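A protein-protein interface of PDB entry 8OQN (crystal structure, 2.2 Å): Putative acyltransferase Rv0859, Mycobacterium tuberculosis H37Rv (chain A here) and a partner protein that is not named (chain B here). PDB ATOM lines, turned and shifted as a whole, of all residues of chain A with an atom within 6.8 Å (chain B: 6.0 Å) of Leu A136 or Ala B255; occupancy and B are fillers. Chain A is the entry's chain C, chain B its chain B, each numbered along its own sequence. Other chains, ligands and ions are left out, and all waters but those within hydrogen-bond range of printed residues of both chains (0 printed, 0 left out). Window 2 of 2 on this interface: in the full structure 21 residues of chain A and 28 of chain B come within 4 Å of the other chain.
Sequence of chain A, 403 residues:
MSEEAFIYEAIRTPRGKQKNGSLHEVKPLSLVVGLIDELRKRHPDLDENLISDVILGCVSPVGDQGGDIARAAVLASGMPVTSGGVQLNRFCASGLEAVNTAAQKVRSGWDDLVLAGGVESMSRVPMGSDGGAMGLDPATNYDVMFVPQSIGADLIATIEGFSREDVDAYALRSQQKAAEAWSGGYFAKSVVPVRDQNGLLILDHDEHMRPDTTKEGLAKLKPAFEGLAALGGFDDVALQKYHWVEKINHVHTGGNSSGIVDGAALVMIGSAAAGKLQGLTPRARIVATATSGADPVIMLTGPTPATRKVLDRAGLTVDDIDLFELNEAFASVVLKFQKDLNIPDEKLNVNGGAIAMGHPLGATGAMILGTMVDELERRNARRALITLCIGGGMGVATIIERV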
ATOM      1  N   GLY A 128      -7.900  -7.795  35.291  1.00  0.00           N
ATOM      2  CA  GLY A 128      -7.423  -8.117  33.965  1.00  0.00           C
ATOM      3  C   GLY A 128      -7.207  -6.928  33.058  1.00  0.00           C
ATOM      4  O   GLY A 128      -6.754  -7.113  31.921  1.00  0.00           O
ATOM      5  N   ASP A 130      -4.912  -4.918  33.077  1.00  0.00           N
ATOM      6  CA  ASP A 130      -3.489  -4.800  32.784  1.00  0.00           C
ATOM      7  C   ASP A 130      -2.986  -5.867  31.823  1.00  0.00           C
ATOM      8  O   ASP A 130      -1.814  -5.822  31.434  1.00  0.00           O
ATOM      9  CB  ASP A 130      -2.683  -4.859  34.083  1.00  0.00           C
ATOM     10  CG  ASP A 130      -2.958  -6.117  34.887  1.00  0.00           C
ATOM     11  OD1 ASP A 130      -4.126  -6.560  34.920  1.00  0.00           O
ATOM     12  OD2 ASP A 130      -2.003  -6.663  35.481  1.00  0.00           O
ATOM     13  N   GLY A 131      -3.832  -6.817  31.430  1.00  0.00           N
ATOM     14  CA  GLY A 131      -3.373  -7.876  30.549  1.00  0.00           C
ATOM     15  C   GLY A 131      -2.492  -8.856  31.299  1.00  0.00           C
ATOM     16  O   GLY A 131      -2.727  -9.174  32.469  1.00  0.00           O
ATOM     17  N   GLY A 132      -1.461  -9.336  30.627  1.00  0.00           N
ATOM     18  CA  GLY A 132      -0.520 -10.271  31.215  1.00  0.00           C
ATOM     19  C   GLY A 132      -0.167 -11.373  30.239  1.00  0.00           C
ATOM     20  O   GLY A 132      -0.863 -11.626  29.257  1.00  0.00           O
ATOM     21  N   ALA A 133       0.947 -12.049  30.521  1.00  0.00           N
ATOM     22  CA  ALA A 133       1.421 -13.106  29.635  1.00  0.00           C
ATOM     23  C   ALA A 133       0.757 -14.440  29.953  1.00  0.00           C
ATOM     24  O   ALA A 133       0.309 -15.148  29.044  1.00  0.00           O
ATOM     25  CB  ALA A 133       2.943 -13.227  29.734  1.00  0.00           C
ATOM     26  N   MET A 134       0.678 -14.789  31.242  1.00  0.00           N
ATOM     27  CA  MET A 134       0.105 -16.063  31.666  1.00  0.00           C
ATOM     28  C   MET A 134      -1.272 -16.320  31.071  1.00  0.00           C
ATOM     29  O   MET A 134      -1.693 -17.480  30.981  1.00  0.00           O
ATOM     30  CB  MET A 134       0.011 -16.111  33.193  1.00  0.00           C
ATOM     31  CG  MET A 134       1.302 -16.481  33.907  1.00  0.00           C
ATOM     32  SD  MET A 134       1.193 -16.179  35.683  1.00  0.00           S
ATOM     33  CE  MET A 134      -0.408 -16.892  36.050  1.00  0.00           C
ATOM     34  N   GLY A 135      -1.983 -15.273  30.664  1.00  0.00           N
ATOM     35  CA  GLY A 135      -3.299 -15.437  30.086  1.00  0.00           C
ATOM     36  C   GLY A 135      -3.359 -15.153  28.599  1.00  0.00           C
ATOM     37  O   GLY A 135      -4.012 -15.885  27.852  1.00  0.00           O
ATOM     38  N   LEU A 136      -2.671 -14.103  28.152  1.00  0.00           N
ATOM     39  CA  LEU A 136      -2.813 -13.627  26.782  1.00  0.00           C
ATOM     40  C   LEU A 136      -1.761 -14.170  25.822  1.00  0.00           C
ATOM     41  O   LEU A 136      -1.988 -14.138  24.608  1.00  0.00           O
ATOM     42  CB  LEU A 136      -2.771 -12.095  26.750  1.00  0.00           C
ATOM     43  CG  LEU A 136      -3.789 -11.377  27.640  1.00  0.00           C
ATOM     44  CD1 LEU A 136      -3.607  -9.871  27.556  1.00  0.00           C
ATOM     45  CD2 LEU A 136      -5.210 -11.764  27.263  1.00  0.00           C
ATOM     46  N   ASP A 137      -0.622 -14.654  26.320  1.00  0.00           N
ATOM     47  CA  ASP A 137       0.412 -15.212  25.455  1.00  0.00           C
ATOM     48  C   ASP A 137       0.146 -16.699  25.255  1.00  0.00           C
ATOM     49  O   ASP A 137       0.286 -17.476  26.213  1.00  0.00           O
ATOM     50  CB  ASP A 137       1.793 -14.987  26.060  1.00  0.00           C
ATOM     51  CG  ASP A 137       2.892 -15.710  25.305  1.00  0.00           C
ATOM     52  OD1 ASP A 137       2.747 -15.926  24.083  1.00  0.00           O
ATOM     53  OD2 ASP A 137       3.902 -16.071  25.945  1.00  0.00           O
ATOM     54  N   PRO A 138      -0.217 -17.145  24.047  1.00  0.00           N
ATOM     55  CA  PRO A 138      -0.674 -18.538  23.892  1.00  0.00           C
ATOM     56  C   PRO A 138       0.372 -19.583  24.229  1.00  0.00           C
ATOM     57  O   PRO A 138       0.028 -20.611  24.824  1.00  0.00           O
ATOM     58  CB  PRO A 138      -1.075 -18.608  22.411  1.00  0.00           C
ATOM     59  CG  PRO A 138      -1.316 -17.200  22.014  1.00  0.00           C
ATOM     60  CD  PRO A 138      -0.335 -16.385  22.794  1.00  0.00           C
ATOM     61  N   ALA A 139       1.636 -19.362  23.857  1.00  0.00           N
ATOM     62  CA  ALA A 139       2.655 -20.388  24.062  1.00  0.00           C
ATOM     63  C   ALA A 139       2.818 -20.726  25.538  1.00  0.00           C
ATOM     64  O   ALA A 139       2.908 -21.903  25.906  1.00  0.00           O
ATOM     65  CB  ALA A 139       3.987 -19.937  23.464  1.00  0.00           C
ATOM     66  N   THR A 140       2.850 -19.713  26.401  1.00  0.00           N
ATOM     67  CA  THR A 140       3.038 -19.958  27.824  1.00  0.00           C
ATOM     68  C   THR A 140       1.734 -20.268  28.546  1.00  0.00           C
ATOM     69  O   THR A 140       1.744 -21.033  29.517  1.00  0.00           O
ATOM     70  CB  THR A 140       3.724 -18.759  28.480  1.00  0.00           C
ATOM     71  OG1 THR A 140       2.891 -17.602  28.352  1.00  0.00           O
ATOM     72  CG2 THR A 140       5.062 -18.489  27.807  1.00  0.00           C
ATOM     73  N   ASN A 141       0.616 -19.683  28.103  1.00  0.00           N
ATOM     74  CA  ASN A 141      -0.693 -20.097  28.603  1.00  0.00           C
ATOM     75  C   ASN A 141      -0.902 -21.590  28.383  1.00  0.00           C
ATOM     76  O   ASN A 141      -1.342 -22.312  29.284  1.00  0.00           O
ATOM     77  CB  ASN A 141      -1.792 -19.283  27.907  1.00  0.00           C
ATOM     78  CG  ASN A 141      -3.198 -19.568  28.445  1.00  0.00           C
ATOM     79  OD1 ASN A 141      -3.490 -20.651  28.953  1.00  0.00           O
ATOM     80  ND2 ASN A 141      -4.082 -18.585  28.313  1.00  0.00           N
ATOM     81  N   LEU A 228     -14.205 -15.290  32.302  1.00  0.00           N
ATOM     82  CA  LEU A 228     -13.373 -16.327  31.682  1.00  0.00           C
ATOM     83  C   LEU A 228     -13.954 -17.723  31.887  1.00  0.00           C
ATOM     84  O   LEU A 228     -13.867 -18.573  30.993  1.00  0.00           O
ATOM     85  CB  LEU A 228     -11.951 -16.248  32.245  1.00  0.00           C
ATOM     86  CG  LEU A 228     -10.816 -15.970  31.259  1.00  0.00           C
ATOM     87  CD1 LEU A 228     -11.142 -14.797  30.349  1.00  0.00           C
ATOM     88  CD2 LEU A 228      -9.543 -15.702  32.031  1.00  0.00           C
ATOM     89  N   THR B 248      -6.964  -6.347  17.572  1.00  0.00           N
ATOM     90  CA  THR B 248      -5.635  -6.807  17.948  1.00  0.00           C
ATOM     91  C   THR B 248      -5.674  -7.391  19.351  1.00  0.00           C
ATOM     92  O   THR B 248      -6.665  -7.244  20.070  1.00  0.00           O
ATOM     93  CB  THR B 248      -4.646  -5.645  17.860  1.00  0.00           C
ATOM     94  OG1 THR B 248      -4.919  -4.703  18.903  1.00  0.00           O
ATOM     95  CG2 THR B 248      -4.756  -4.951  16.511  1.00  0.00           C
ATOM     96  N   PRO B 249      -4.617  -8.094  19.773  1.00  0.00           N
ATOM     97  CA  PRO B 249      -4.599  -8.600  21.156  1.00  0.00           C
ATOM     98  C   PRO B 249      -4.736  -7.511  22.205  1.00  0.00           C
ATOM     99  O   PRO B 249      -5.274  -7.772  23.289  1.00  0.00           O
ATOM    100  CB  PRO B 249      -3.241  -9.308  21.247  1.00  0.00           C
ATOM    101  CG  PRO B 249      -2.965  -9.743  19.857  1.00  0.00           C
ATOM    102  CD  PRO B 249      -3.515  -8.657  18.971  1.00  0.00           C
ATOM    103  N   SER B 250      -4.271  -6.296  21.919  1.00  0.00           N
ATOM    104  CA  SER B 250      -4.426  -5.181  22.845  1.00  0.00           C
ATOM    105  C   SER B 250      -5.804  -4.537  22.771  1.00  0.00           C
ATOM    106  O   SER B 250      -6.068  -3.590  23.520  1.00  0.00           O
ATOM    107  CB  SER B 250      -3.346  -4.128  22.584  1.00  0.00           C
ATOM    108  OG  SER B 250      -3.430  -3.628  21.263  1.00  0.00           O
ATOM    109  N   SER B 251      -6.682  -5.017  21.887  1.00  0.00           N
ATOM    110  CA  SER B 251      -8.049  -4.525  21.840  1.00  0.00           C
ATOM    111  C   SER B 251      -8.861  -5.143  22.977  1.00  0.00           C
ATOM    112  O   SER B 251      -8.770  -6.349  23.216  1.00  0.00           O
ATOM    113  CB  SER B 251      -8.699  -4.858  20.496  1.00  0.00           C
ATOM    114  OG  SER B 251     -10.045  -4.415  20.454  1.00  0.00           O
ATOM    115  N   PRO B 252      -9.659  -4.341  23.686  1.00  0.00           N
ATOM    116  CA  PRO B 252     -10.352  -4.865  24.877  1.00  0.00           C
ATOM    117  C   PRO B 252     -11.335  -5.982  24.572  1.00  0.00           C
ATOM    118  O   PRO B 252     -11.501  -6.888  25.398  1.00  0.00           O
ATOM    119  CB  PRO B 252     -11.063  -3.626  25.438  1.00  0.00           C
ATOM    120  CG  PRO B 252     -11.219  -2.716  24.267  1.00  0.00           C
ATOM    121  CD  PRO B 252     -10.012  -2.938  23.407  1.00  0.00           C
ATOM    122  N   GLY B 253     -11.993  -5.949  23.414  1.00  0.00           N
ATOM    123  CA  GLY B 253     -12.926  -7.015  23.085  1.00  0.00           C
ATOM    124  C   GLY B 253     -12.229  -8.346  22.876  1.00  0.00           C
ATOM    125  O   GLY B 253     -12.684  -9.386  23.358  1.00  0.00           O
ATOM    126  N   LEU B 254     -11.109  -8.329  22.152  1.00  0.00           N
ATOM    127  CA  LEU B 254     -10.380  -9.568  21.909  1.00  0.00           C
ATOM    128  C   LEU B 254      -9.612 -10.016  23.145  1.00  0.00           C
ATOM    129  O   LEU B 254      -9.440 -11.220  23.367  1.00  0.00           O
ATOM    130  CB  LEU B 254      -9.438  -9.395  20.720  1.00  0.00           C
ATOM    131  CG  LEU B 254      -8.695 -10.647  20.249  1.00  0.00           C
ATOM    132  CD1 LEU B 254      -9.680 -11.685  19.735  1.00  0.00           C
ATOM    133  CD2 LEU B 254      -7.662 -10.304  19.182  1.00  0.00           C
ATOM    134  N   ALA B 255      -9.155  -9.067  23.966  1.00  0.00           N
ATOM    135  CA  ALA B 255      -8.410  -9.419  25.169  1.00  0.00           C
ATOM    136  C   ALA B 255      -9.264 -10.178  26.173  1.00  0.00           C
ATOM    137  O   ALA B 255      -8.719 -10.900  27.014  1.00  0.00           O
ATOM    138  CB  ALA B 255      -7.843  -8.159  25.819  1.00  0.00           C
ATOM    139  N   ALA B 256     -10.586 -10.036  26.097  1.00  0.00           N
ATOM    140  CA  ALA B 256     -11.455 -10.701  27.059  1.00  0.00           C
ATOM    141  C   ALA B 256     -11.556 -12.195  26.775  1.00  0.00           C
ATOM    142  O   ALA B 256     -11.651 -13.001  27.707  1.00  0.00           O
ATOM    143  CB  ALA B 256     -12.840 -10.058  27.056  1.00  0.00           C
ATOM    144  N   ILE B 257     -11.537 -12.585  25.501  1.00  0.00           N
ATOM    145  CA  ILE B 257     -11.677 -13.992  25.138  1.00  0.00           C
ATOM    146  C   ILE B 257     -10.345 -14.663  24.822  1.00  0.00           C
ATOM    147  O   ILE B 257     -10.286 -15.901  24.780  1.00  0.00           O
ATOM    148  CB  ILE B 257     -12.642 -14.157  23.947  1.00  0.00           C
ATOM    149  CG1 ILE B 257     -12.075 -13.462  22.708  1.00  0.00           C
ATOM    150  CG2 ILE B 257     -14.019 -13.614  24.300  1.00  0.00           C
ATOM    151  CD1 ILE B 257     -12.942 -13.626  21.484  1.00  0.00           C
ATOM    152  N   LEU B 258      -9.282 -13.891  24.611  1.00  0.00           N
ATOM    153  CA  LEU B 258      -7.995 -14.465  24.227  1.00  0.00           C
ATOM    154  C   LEU B 258      -7.459 -15.519  25.193  1.00  0.00           C
ATOM    155  O   LEU B 258      -6.907 -16.523  24.711  1.00  0.00           O
ATOM    156  CB  LEU B 258      -6.975 -13.332  24.040  1.00  0.00           C
ATOM    157  CG  LEU B 258      -5.895 -13.545  22.977  1.00  0.00           C
ATOM    158  CD1 LEU B 258      -6.534 -13.972  21.669  1.00  0.00           C
ATOM    159  CD2 LEU B 258      -5.089 -12.272  22.778  1.00  0.00           C
ATOM    160  N   PRO B 259      -7.568 -15.376  26.520  1.00  0.00           N
ATOM    161  CA  PRO B 259      -7.055 -16.437  27.406  1.00  0.00           C
ATOM    162  C   PRO B 259      -7.722 -17.787  27.211  1.00  0.00           C
ATOM    163  O   PRO B 259      -7.153 -18.802  27.631  1.00  0.00           O
ATOM    164  CB  PRO B 259      -7.323 -15.883  28.812  1.00  0.00           C
ATOM    165  CG  PRO B 259      -7.348 -14.413  28.633  1.00  0.00           C
ATOM    166  CD  PRO B 259      -7.986 -14.191  27.296  1.00  0.00           C
ATOM    167  N   VAL B 285      -0.935 -15.040  17.274  1.00  0.00           N
ATOM    168  CA  VAL B 285      -1.188 -13.990  18.256  1.00  0.00           C
ATOM    169  C   VAL B 285       0.036 -13.098  18.419  1.00  0.00           C
ATOM    170  O   VAL B 285      -0.079 -11.866  18.473  1.00  0.00           O
ATOM    171  CB  VAL B 285      -1.625 -14.606  19.594  1.00  0.00           C
ATOM    172  CG1 VAL B 285      -1.761 -13.526  20.647  1.00  0.00           C
ATOM    173  CG2 VAL B 285      -2.938 -15.348  19.419  1.00  0.00           C
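Pro B259 touches Gly A135. Ala B255 touches Leu A136. CD2 of Leu A136 touches CB of Leu B258, 3.995 Å away. Leu A136 touches Pro B259. Pro A138 touches Val B285. Leu A228 touches Ala B256. CD2 of Leu A228 touches CB of Pro B259 (3.9 Å).
The backbone carbonyl oxygen (O) of Gly A135 sits at hydrogen-bond distance from the side-chain amide nitrogen (ND2) of Asn A141 (2.7 Å).
O of Pro B259 sits at hydrogen-bond distance from ND2 of Asn A141 (3.2 Å).
Gly A128 touches none of the printed residues of chain B. Printed residues of chain B within 4 Å of Pro A138: Val B285 (3.6 Å). Printed residues of chain B within 4 Å of Leu A228: Ala B256 (3.2 Å) and Pro B259 (3.9 Å). Leu B254 touches none of the printed residues of chain A. Ala B255 touches just one residue of chain A: Leu A136 (3.6 Å). Printed residues of chain A within 4 Å of Ala B256: Leu A228 (3.2 Å). The nearest printed residue of chain B that does not touch Leu A136 is Val B285 (4.01 Å). The nearest residue of chain A that does not touch Ala B255 is Leu A228 (5.7 Å).
Of the 14 printed residues of chain A, 5 touch a printed residue of chain B. Printed residues of chain A that touch a printed residue of chain B: Gly A135, Leu A136, Pro A138, Asn A141 and Leu A228. Along chain A the printed residues that touch a printed residue of chain B span positions 135 to 228. Of the 13 printed residues of chain B, 5 touch a printed residue of chain A. Hydrophobic or aromatic side chains of chain B within 4 Å of the printed part of chain A: Leu B258, Pro B259 and Val B285. Among the printed residues, 8 pairs touch across the chains.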
